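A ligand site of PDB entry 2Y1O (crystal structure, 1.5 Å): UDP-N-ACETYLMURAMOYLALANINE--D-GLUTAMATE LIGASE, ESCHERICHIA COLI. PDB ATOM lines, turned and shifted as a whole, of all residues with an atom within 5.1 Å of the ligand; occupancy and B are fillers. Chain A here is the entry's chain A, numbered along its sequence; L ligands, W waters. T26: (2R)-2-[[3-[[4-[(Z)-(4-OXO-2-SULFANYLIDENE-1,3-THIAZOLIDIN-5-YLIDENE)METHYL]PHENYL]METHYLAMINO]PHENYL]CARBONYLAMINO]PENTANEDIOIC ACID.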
ATOM      1  N   ILE A  12     -36.427   7.638  10.966  1.00  0.00           N
ATOM      2  CA  ILE A  12     -36.737   8.949  11.535  1.00  0.00           C
ATOM      3  C   ILE A  12     -35.692   9.936  11.051  1.00  0.00           C
ATOM      4  O   ILE A  12     -34.505   9.784  11.355  1.00  0.00           O
ATOM      5  CB  ILE A  12     -36.646   8.925  13.055  1.00  0.00           C
ATOM      6  CG1 ILE A  12     -37.293   7.634  13.579  1.00  0.00           C
ATOM      7  CG2 ILE A  12     -37.308  10.184  13.646  1.00  0.00           C
ATOM      8  CD1 ILE A  12     -38.763   7.709  13.464  1.00  0.00           C
ATOM      9  N   GLY A  13     -36.152  10.945  10.328  1.00  0.00           N
ATOM     10  CA  GLY A  13     -35.298  12.014   9.790  1.00  0.00           C
ATOM     11  C   GLY A  13     -34.973  11.794   8.326  1.00  0.00           C
ATOM     12  O   GLY A  13     -34.446  10.727   7.950  1.00  0.00           O
ATOM     13  N   MET A  35     -40.610   9.103   8.999  1.00  0.00           N
ATOM     14  CA  MET A  35     -41.208  10.195   9.748  1.00  0.00           C
ATOM     15  C   MET A  35     -40.172  11.280  10.026  1.00  0.00           C
ATOM     16  O   MET A  35     -38.968  10.994  10.070  1.00  0.00           O
ATOM     17  CB  MET A  35     -41.870   9.723  11.051  1.00  0.00           C
ATOM     18  CG  MET A  35     -40.913   9.100  12.048  1.00  0.00           C
ATOM     19  SD  MET A  35     -41.798   8.499  13.515  1.00  0.00           S
ATOM     20  CE  MET A  35     -42.783   7.194  12.791  1.00  0.00           C
ATOM     21  N   ASP A  36     -40.645  12.500  10.204  1.00  0.00           N
ATOM     22  CA  ASP A  36     -39.745  13.626  10.502  1.00  0.00           C
ATOM     23  C   ASP A  36     -40.576  14.676  11.263  1.00  0.00           C
ATOM     24  O   ASP A  36     -41.735  14.938  10.898  1.00  0.00           O
ATOM     25  CB  ASP A  36     -39.178  14.165   9.166  1.00  0.00           C
ATOM     26  CG  ASP A  36     -37.980  15.104   9.356  1.00  0.00           C
ATOM     27  OD1 ASP A  36     -38.069  16.108  10.083  1.00  0.00           O
ATOM     28  OD2 ASP A  36     -36.906  14.803   8.780  1.00  0.00           O
ATOM     29  N   THR A  37     -40.020  15.250  12.327  1.00  0.00           N
ATOM     30  CA  THR A  37     -40.781  16.248  13.092  1.00  0.00           C
ATOM     31  C   THR A  37     -40.938  17.571  12.336  1.00  0.00           C
ATOM     32  O   THR A  37     -41.809  18.385  12.677  1.00  0.00           O
ATOM     33  CB  THR A  37     -40.108  16.584  14.468  1.00  0.00           C
ATOM     34  OG1 THR A  37     -38.824  17.155  14.213  1.00  0.00           O
ATOM     35  CG2 THR A  37     -39.903  15.329  15.344  1.00  0.00           C
ATOM     36  N   ARG A  38     -40.125  17.787  11.307  1.00  0.00           N
ATOM     37  CA  ARG A  38     -40.276  18.958  10.425  1.00  0.00           C
ATOM     38  C   ARG A  38     -41.417  18.735   9.423  1.00  0.00           C
ATOM     39  O   ARG A  38     -41.560  17.635   8.885  1.00  0.00           O
ATOM     40  CB  ARG A  38     -38.960  19.231   9.691  1.00  0.00           C
ATOM     41  CG  ARG A  38     -37.793  19.564  10.669  1.00  0.00           C
ATOM     42  CD  ARG A  38     -36.418  19.532   9.978  1.00  0.00           C
ATOM     43  NE  ARG A  38     -36.055  18.185   9.535  1.00  0.00           N
ATOM     44  CZ  ARG A  38     -34.902  17.862   8.954  1.00  0.00           C
ATOM     45  NH1 ARG A  38     -33.947  18.781   8.771  1.00  0.00           N
ATOM     46  NH2 ARG A  38     -34.685  16.596   8.585  1.00  0.00           N
ATOM     47  N   LEU A  58     -43.552  13.035  15.300  1.00  0.00           N
ATOM     48  CA  LEU A  58     -43.334  11.589  15.245  1.00  0.00           C
ATOM     49  C   LEU A  58     -44.684  10.916  15.432  1.00  0.00           C
ATOM     50  O   LEU A  58     -45.616  11.488  16.025  1.00  0.00           O
ATOM     51  CB  LEU A  58     -42.396  11.160  16.374  1.00  0.00           C
ATOM     52  CG  LEU A  58     -41.000  11.790  16.317  1.00  0.00           C
ATOM     53  CD1 LEU A  58     -40.105  11.163  17.374  1.00  0.00           C
ATOM     54  CD2 LEU A  58     -40.366  11.614  14.938  1.00  0.00           C
ATOM     55  N   SER A  72     -31.990   9.198  12.584  1.00  0.00           N
ATOM     56  CA  SER A  72     -31.031  10.238  12.178  1.00  0.00           C
ATOM     57  C   SER A  72     -30.201  10.638  13.391  1.00  0.00           C
ATOM     58  O   SER A  72     -30.715  10.720  14.504  1.00  0.00           O
ATOM     59  CB  SER A  72     -31.803  11.491  11.732  1.00  0.00           C
ATOM     60  OG  SER A  72     -30.909  12.603  11.599  1.00  0.00           O
ATOM     61  N   PRO A  73     -28.931  10.977  13.181  1.00  0.00           N
ATOM     62  CA  PRO A  73     -28.242  11.573  14.313  1.00  0.00           C
ATOM     63  C   PRO A  73     -28.810  12.916  14.784  1.00  0.00           C
ATOM     64  O   PRO A  73     -28.416  13.405  15.854  1.00  0.00           O
ATOM     65  CB  PRO A  73     -26.799  11.736  13.786  1.00  0.00           C
ATOM     66  CG  PRO A  73     -26.929  11.838  12.297  1.00  0.00           C
ATOM     67  CD  PRO A  73     -28.093  10.877  11.973  1.00  0.00           C
ATOM     68  N   GLY A  74     -29.711  13.539  14.029  1.00  0.00           N
ATOM     69  CA  GLY A  74     -30.304  14.801  14.447  1.00  0.00           C
ATOM     70  C   GLY A  74     -31.496  14.641  15.397  1.00  0.00           C
ATOM     71  O   GLY A  74     -32.034  15.663  15.864  1.00  0.00           O
ATOM     72  N   ILE A  75     -31.902  13.413  15.706  1.00  0.00           N
ATOM     73  CA  ILE A  75     -32.949  13.199  16.746  1.00  0.00           C
ATOM     74  C   ILE A  75     -32.353  12.555  17.993  1.00  0.00           C
ATOM     75  O   ILE A  75     -31.678  11.513  17.941  1.00  0.00           O
ATOM     76  CB  ILE A  75     -34.174  12.399  16.213  1.00  0.00           C
ATOM     77  CG1 ILE A  75     -35.214  12.283  17.345  1.00  0.00           C
ATOM     78  CG2 ILE A  75     -33.781  10.996  15.821  1.00  0.00           C
ATOM     79  CD1 ILE A  75     -36.620  12.547  16.916  1.00  0.00           C
ATOM     80  N   LYS A 116     -11.809  16.648  12.868  1.00  0.00           N
ATOM     81  CA  LYS A 116     -12.117  15.320  12.372  1.00  0.00           C
ATOM     82  C   LYS A 116     -12.335  15.294  10.845  1.00  0.00           C
ATOM     83  O   LYS A 116     -11.932  14.327  10.199  1.00  0.00           O
ATOM     84  CB  LYS A 116     -13.260  14.660  13.143  1.00  0.00           C
ATOM     85  CG  LYS A 116     -14.551  15.386  13.120  1.00  0.00           C
ATOM     86  CD  LYS A 116     -15.603  14.606  13.972  1.00  0.00           C
ATOM     87  CE  LYS A 116     -16.982  15.252  13.886  1.00  0.00           C
ATOM     88  NZ  LYS A 116     -16.993  16.597  14.484  1.00  0.00           N
ATOM     89  N   ILE A 140     -22.205  15.318   6.855  1.00  0.00           N
ATOM     90  CA  ILE A 140     -23.474  15.770   6.269  1.00  0.00           C
ATOM     91  C   ILE A 140     -23.593  15.603   4.742  1.00  0.00           C
ATOM     92  O   ILE A 140     -24.628  15.150   4.252  1.00  0.00           O
ATOM     93  CB  ILE A 140     -23.785  17.241   6.675  1.00  0.00           C
ATOM     94  CG1 ILE A 140     -24.012  17.325   8.190  1.00  0.00           C
ATOM     95  CG2 ILE A 140     -25.007  17.766   5.936  1.00  0.00           C
ATOM     96  CD1 ILE A 140     -24.724  16.112   8.797  1.00  0.00           C
ATOM     97  N   PHE A 162     -23.053  11.770  17.920  1.00  0.00           N
ATOM     98  CA  PHE A 162     -24.439  11.350  17.737  1.00  0.00           C
ATOM     99  C   PHE A 162     -24.515  10.027  16.957  1.00  0.00           C
ATOM    100  O   PHE A 162     -25.276   9.106  17.308  1.00  0.00           O
ATOM    101  CB  PHE A 162     -25.217  12.458  16.982  1.00  0.00           C
ATOM    102  CG  PHE A 162     -25.234  13.766  17.706  1.00  0.00           C
ATOM    103  CD1 PHE A 162     -25.482  13.840  19.051  1.00  0.00           C
ATOM    104  CD2 PHE A 162     -24.960  14.933  17.019  1.00  0.00           C
ATOM    105  CE1 PHE A 162     -25.498  15.046  19.737  1.00  0.00           C
ATOM    106  CE2 PHE A 162     -24.948  16.166  17.695  1.00  0.00           C
ATOM    107  CZ  PHE A 162     -25.225  16.205  19.061  1.00  0.00           C
ATOM    108  N   ASP A 183     -18.921  20.746  23.577  1.00  0.00           N
ATOM    109  CA  ASP A 183     -19.815  20.994  22.424  1.00  0.00           C
ATOM    110  C   ASP A 183     -21.085  20.163  22.593  1.00  0.00           C
ATOM    111  O   ASP A 183     -21.129  19.215  23.399  1.00  0.00           O
ATOM    112  CB  ASP A 183     -19.073  20.595  21.127  1.00  0.00           C
ATOM    113  CG  ASP A 183     -19.721  21.140  19.862  1.00  0.00           C
ATOM    114  OD1 ASP A 183     -20.666  21.943  19.959  1.00  0.00           O
ATOM    115  OD2 ASP A 183     -19.244  20.750  18.754  1.00  0.00           O
ATOM    116  N   HIS A 184     -22.102  20.534  21.822  1.00  0.00           N
ATOM    117  CA  HIS A 184     -23.359  19.767  21.795  1.00  0.00           C
ATOM    118  C   HIS A 184     -24.003  19.619  23.170  1.00  0.00           C
ATOM    119  O   HIS A 184     -24.685  18.624  23.406  1.00  0.00           O
ATOM    120  CB  HIS A 184     -23.137  18.381  21.177  1.00  0.00           C
ATOM    121  CG  HIS A 184     -22.500  18.420  19.804  1.00  0.00           C
ATOM    122  ND1 HIS A 184     -23.087  19.079  18.747  1.00  0.00           N
ATOM    123  CD2 HIS A 184     -21.377  17.847  19.333  1.00  0.00           C
ATOM    124  CE1 HIS A 184     -22.348  18.901  17.664  1.00  0.00           C
ATOM    125  NE2 HIS A 184     -21.305  18.147  17.987  1.00  0.00           N
ATOM    126  N   ARG A 187     -27.589  18.613  23.641  1.00  0.00           N
ATOM    127  CA  ARG A 187     -27.921  17.186  23.459  1.00  0.00           C
ATOM    128  C   ARG A 187     -27.348  16.272  24.532  1.00  0.00           C
ATOM    129  O   ARG A 187     -27.627  15.074  24.531  1.00  0.00           O
ATOM    130  CB  ARG A 187     -27.427  16.631  22.094  1.00  0.00           C
ATOM    131  CG  ARG A 187     -28.297  17.067  20.926  1.00  0.00           C
ATOM    132  CD  ARG A 187     -29.443  16.098  20.673  1.00  0.00           C
ATOM    133  NE  ARG A 187     -29.082  14.722  20.309  1.00  0.00           N
ATOM    134  CZ  ARG A 187     -28.949  14.312  19.045  1.00  0.00           C
ATOM    135  NH1 ARG A 187     -29.063  15.214  18.072  1.00  0.00           N
ATOM    136  NH2 ARG A 187     -28.651  13.047  18.783  1.00  0.00           N
ATOM    137  N   LYS A 320     -16.437  26.811   9.741  1.00  0.00           N
ATOM    138  CA  LYS A 320     -16.519  25.475  10.364  1.00  0.00           C
ATOM    139  C   LYS A 320     -16.188  25.499  11.870  1.00  0.00           C
ATOM    140  O   LYS A 320     -16.358  24.477  12.566  1.00  0.00           O
ATOM    141  CB  LYS A 320     -15.637  24.500   9.592  1.00  0.00           C
ATOM    142  CG  LYS A 320     -15.710  23.013  10.051  1.00  0.00           C
ATOM    143  CD  LYS A 320     -17.106  22.420  10.178  1.00  0.00           C
ATOM    144  CE  LYS A 320     -17.040  20.977  10.743  1.00  0.00           C
ATOM    145  NZ  LYS A 320     -18.368  20.361  11.074  1.00  0.00           N
ATOM    146  N   THR A 322     -17.631  25.771  14.857  1.00  0.00           N
ATOM    147  CA  THR A 322     -18.999  25.738  15.384  1.00  0.00           C
ATOM    148  C   THR A 322     -18.990  25.472  16.893  1.00  0.00           C
ATOM    149  O   THR A 322     -20.039  25.223  17.494  1.00  0.00           O
ATOM    150  CB  THR A 322     -19.810  24.628  14.675  1.00  0.00           C
ATOM    151  OG1 THR A 322     -19.111  23.392  14.799  1.00  0.00           O
ATOM    152  CG2 THR A 322     -19.939  24.966  13.161  1.00  0.00           C
ATOM    153  N   LYS A 349     -25.398  26.669  21.681  1.00  0.00           N
ATOM    154  CA  LYS A 349     -25.707  25.348  22.242  1.00  0.00           C
ATOM    155  C   LYS A 349     -25.405  25.277  23.730  1.00  0.00           C
ATOM    156  O   LYS A 349     -24.970  24.231  24.195  1.00  0.00           O
ATOM    157  CB  LYS A 349     -24.860  24.275  21.550  1.00  0.00           C
ATOM    158  CG  LYS A 349     -25.332  23.950  20.150  1.00  0.00           C
ATOM    159  CD  LYS A 349     -24.260  23.178  19.420  1.00  0.00           C
ATOM    160  CE  LYS A 349     -23.215  24.142  18.787  1.00  0.00           C
ATOM    161  NZ  LYS A 349     -22.272  23.297  18.022  1.00  0.00           N
ATOM    162  N   CYS A 414     -20.133  28.869  17.203  1.00  0.00           N
ATOM    163  CA  CYS A 414     -21.540  28.488  17.366  1.00  0.00           C
ATOM    164  C   CYS A 414     -21.995  27.760  16.141  1.00  0.00           C
ATOM    165  O   CYS A 414     -21.435  27.929  15.051  1.00  0.00           O
ATOM    166  CB  CYS A 414     -22.436  29.719  17.504  1.00  0.00           C
ATOM    167  SG  CYS A 414     -22.072  30.806  18.839  1.00  0.00           S
ATOM    168  N   ALA A 415     -23.041  26.949  16.298  1.00  0.00           N
ATOM    169  CA  ALA A 415     -23.696  26.383  15.141  1.00  0.00           C
ATOM    170  C   ALA A 415     -24.425  27.487  14.343  1.00  0.00           C
ATOM    171  O   ALA A 415     -24.776  28.540  14.883  1.00  0.00           O
ATOM    172  CB  ALA A 415     -24.713  25.304  15.560  1.00  0.00           C
ATOM    173  N   SER A 416     -24.648  27.206  13.065  1.00  0.00           N
ATOM    174  CA  SER A 416     -25.265  28.178  12.166  1.00  0.00           C
ATOM    175  C   SER A 416     -26.749  27.928  12.025  1.00  0.00           C
ATOM    176  O   SER A 416     -27.432  28.636  11.303  1.00  0.00           O
ATOM    177  CB  SER A 416     -24.643  28.079  10.767  1.00  0.00           C
ATOM    178  OG  SER A 416     -25.038  26.874  10.128  1.00  0.00           O
ATOM    179  N   LEU A 417     -27.253  26.886  12.717  1.00  0.00           N
ATOM    180  CA  LEU A 417     -28.549  26.325  12.383  1.00  0.00           C
ATOM    181  C   LEU A 417     -29.726  27.257  12.737  1.00  0.00           C
ATOM    182  O   LEU A 417     -30.858  27.041  12.319  1.00  0.00           O
ATOM    183  CB  LEU A 417     -28.717  24.951  13.025  1.00  0.00           C
ATOM    184  CG  LEU A 417     -27.601  23.976  12.624  1.00  0.00           C
ATOM    185  CD1 LEU A 417     -27.796  22.589  13.196  1.00  0.00           C
ATOM    186  CD2 LEU A 417     -27.466  23.899  11.121  1.00  0.00           C
ATOM    187  N   ASN A 422     -26.745  25.260   7.214  1.00  0.00           N
ATOM    188  CA  ASN A 422     -25.534  24.644   7.745  1.00  0.00           C
ATOM    189  C   ASN A 422     -24.348  25.610   7.601  1.00  0.00           C
ATOM    190  O   ASN A 422     -24.478  26.688   6.971  1.00  0.00           O
ATOM    191  CB  ASN A 422     -25.244  23.299   7.060  1.00  0.00           C
ATOM    192  CG  ASN A 422     -25.106  23.438   5.561  1.00  0.00           C
ATOM    193  OD1 ASN A 422     -24.307  24.239   5.096  1.00  0.00           O
ATOM    194  ND2 ASN A 422     -25.916  22.699   4.802  1.00  0.00           N
ATOM    195  N   PHE A 423     -23.205  25.223   8.184  1.00  0.00           N
ATOM    196  CA  PHE A 423     -22.053  26.114   8.270  1.00  0.00           C
ATOM    197  C   PHE A 423     -21.479  26.396   6.876  1.00  0.00           C
ATOM    198  O   PHE A 423     -20.803  27.417   6.698  1.00  0.00           O
ATOM    199  CB  PHE A 423     -20.956  25.512   9.186  1.00  0.00           C
ATOM    200  CG  PHE A 423     -20.255  24.320   8.564  1.00  0.00           C
ATOM    201  CD1 PHE A 423     -20.782  23.036   8.741  1.00  0.00           C
ATOM    202  CD2 PHE A 423     -19.140  24.490   7.759  1.00  0.00           C
ATOM    203  CE1 PHE A 423     -20.178  21.911   8.124  1.00  0.00           C
ATOM    204  CE2 PHE A 423     -18.505  23.382   7.152  1.00  0.00           C
ATOM    205  CZ  PHE A 423     -19.039  22.091   7.331  1.00  0.00           C
ATOM    206  N   ARG A 426     -23.352  29.317   5.582  1.00  0.00           N
ATOM    207  CA  ARG A 426     -22.854  30.490   6.294  1.00  0.00           C
ATOM    208  C   ARG A 426     -21.511  30.962   5.713  1.00  0.00           C
ATOM    209  O   ARG A 426     -21.282  32.159   5.481  1.00  0.00           O
ATOM    210  CB  ARG A 426     -22.824  30.210   7.823  1.00  0.00           C
ATOM    211  CG  ARG A 426     -22.196  31.311   8.653  1.00  0.00           C
ATOM    212  CD  ARG A 426     -22.210  30.991  10.150  1.00  0.00           C
ATOM    213  NE  ARG A 426     -21.343  29.860  10.509  1.00  0.00           N
ATOM    214  CZ  ARG A 426     -21.368  29.306  11.715  1.00  0.00           C
ATOM    215  NH1 ARG A 426     -22.229  29.751  12.641  1.00  0.00           N
ATOM    216  NH2 ARG A 426     -20.558  28.285  11.981  1.00  0.00           N
HETATM  217  OE2 T26 L   1     -23.666  23.339  10.314  1.00  0.00           O
HETATM  218  CD  T26 L   1     -23.616  23.781  11.486  1.00  0.00           C
HETATM  219  OE1 T26 L   1     -23.565  25.022  11.709  1.00  0.00           O
HETATM  220  CG  T26 L   1     -23.676  22.837  12.674  1.00  0.00           C
HETATM  221  CB  T26 L   1     -22.487  21.863  12.733  1.00  0.00           C
HETATM  222  C   T26 L   1     -21.526  19.811  13.785  1.00  0.00           C
HETATM  223  OXT T26 L   1     -21.213  19.086  12.787  1.00  0.00           O
HETATM  224  O   T26 L   1     -20.854  19.851  14.847  1.00  0.00           O
HETATM  225  N   T26 L   1     -23.902  19.945  13.231  1.00  0.00           N
HETATM  226  CAU T26 L   1     -24.743  19.284  14.021  1.00  0.00           C
HETATM  227  OBC T26 L   1     -24.742  19.486  15.233  1.00  0.00           O
HETATM  228  CAT T26 L   1     -25.646  18.258  13.461  1.00  0.00           C
HETATM  229  CAS T26 L   1     -26.044  18.308  12.183  1.00  0.00           C
HETATM  230  CAQ T26 L   1     -26.105  17.121  14.293  1.00  0.00           C
HETATM  231  CAR T26 L   1     -26.788  17.281  11.610  1.00  0.00           C
HETATM  232  CAO T26 L   1     -26.837  16.089  13.699  1.00  0.00           C
HETATM  233  CAP T26 L   1     -27.248  16.206  12.374  1.00  0.00           C
HETATM  234  CAA T26 L   1     -29.547  16.872  10.194  1.00  0.00           C
HETATM  235  CAN T26 L   1     -28.242  16.623   9.550  1.00  0.00           C
HETATM  236  NAY T26 L   1     -27.077  17.341  10.172  1.00  0.00           N
HETATM  237  CAC T26 L   1     -29.951  18.179  10.447  1.00  0.00           C
HETATM  238  CAE T26 L   1     -31.158  18.414  11.075  1.00  0.00           C
HETATM  239  CAB T26 L   1     -30.370  15.822  10.538  1.00  0.00           C
HETATM  240  CAG T26 L   1     -31.595  16.058  11.166  1.00  0.00           C
HETATM  241  CAF T26 L   1     -32.010  17.365  11.426  1.00  0.00           C
HETATM  242  CAH T26 L   1     -33.286  17.684  12.106  1.00  0.00           C
HETATM  243  CAI T26 L   1     -34.305  16.872  12.414  1.00  0.00           C
HETATM  244  SBG T26 L   1     -34.424  15.133  12.227  1.00  0.00           S
HETATM  245  CAL T26 L   1     -36.042  15.248  12.847  1.00  0.00           C
HETATM  246  SBH T26 L   1     -36.968  13.749  13.021  1.00  0.00           S
HETATM  247  NAX T26 L   1     -36.518  16.462  13.253  1.00  0.00           N
HETATM  248  CAK T26 L   1     -35.559  17.381  12.996  1.00  0.00           C
HETATM  249  CA  T26 L   1     -22.737  20.707  13.731  1.00  0.00           C
HETATM  250  OBE T26 L   1     -35.725  18.631  13.258  1.00  0.00           O
HETATM  251  O   HOH W   1     -26.907  19.595  16.953  1.00  0.00           O
HETATM  252  O   HOH W   2     -19.846  16.802  13.365  1.00  0.00           O
HETATM  253  O   HOH W   3     -20.293  21.748  16.494  1.00  0.00           O
HETATM  254  O   HOH W   4     -24.405  21.866  16.636  1.00  0.00           O
HETATM  255  O   HOH W   5     -31.928  16.504   7.551  1.00  0.00           O
HETATM  256  O   HOH W   6     -24.400  20.837   9.889  1.00  0.00           O
HETATM  257  O   HOH W   7     -18.147  19.335  15.114  1.00  0.00           O
HETATM  258  O   HOH W   8     -26.835  20.126   8.895  1.00  0.00           O
HETATM  259  O   HOH W   9     -22.443  18.862  10.281  1.00  0.00           O
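The backbone carbonyl oxygen of Asn 422 sits close to the side-chain hydroxyl of Ser 416 (3.2 Å). A ring nitrogen (NE2) of His 184 is in hydrogen-bond range of the side-chain carboxylate of Asp 183 (3.4 Å). The backbone NH (N) of Ser 72 is in hydrogen-bond range of the backbone carbonyl oxygen (O) of Ile 12 (2.9 Å). The side-chain hydroxyl of Ser 72 sits at hydrogen-bond distance from the backbone NH of Gly 74. The guanidinium group (NH2) of Arg 38 is in salt-bridge range of the side-chain carboxylate (OD2) of Asp 36 (2.9 Å). NH1 of Arg 187 sits at hydrogen-bond distance from O of Pro 73 (2.9 Å). O of Thr 322 sits at hydrogen-bond distance from NZ of Lys 349 (3.0 Å). The backbone carbonyl oxygen (O) of Met 35 is in hydrogen-bond range of the backbone NH (N) of Gly 13 (2.8 Å).
The backbone NH of Thr 37 sits close to a sulfur (SBH) of the ligand, 3.5 Å away. OG1 of Thr 37 lies within hydrogen-bond range of NAX of the ligand, 2.6 Å away. N of Ser 416 sits at hydrogen-bond distance from OE1 of the ligand (2.8 Å). The side-chain hydroxyl of Ser 416 is in hydrogen-bond range of an oxygen (OE1) of the ligand. An oxygen (OE2) of the ligand lies within hydrogen-bond range of the backbone NH (N) of Phe 423 (2.9 Å). NZ of Lys 320 lies within salt-bridge range of OXT of the ligand.
Water W3 lies within hydrogen-bond range of O of the ligand (2.6 Å), OG1 of Thr 322 (2.6 Å), OD2 of Asp 183 (2.7 Å) and NZ of Lys 349 (2.9 Å). Water W2 lies within hydrogen-bond range of OXT of the ligand (2.7 Å) and NZ of Lys 116 (3.1 Å). Water W7 lies within hydrogen-bond range of an oxygen (O) of the ligand (2.8 Å) and the side-chain amino group (NZ) of Lys 116 (3.0 Å). Water W4 bridges an oxygen (OBC) of the ligand (2.8 Å) and the side-chain amino group of Lys 349 (2.9 Å).
Residues that only touch the ligand: Ile 12 (3.6 Å), Gly 13 (3.97 Å), Asp 36 (3.5 Å), Arg 38 (3.4 Å), Ser 72 (3.4 Å), Pro 73 (3.8 Å), Gly 74 (3.7 Å), Ile 140 (3.0 Å), Phe 162 (3.7 Å), His 184 (3.3 Å), Thr 322 (3.9 Å), Ala 415 (3.7 Å), Leu 417 (3.9 Å) and Asn 422 (3.4 Å).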
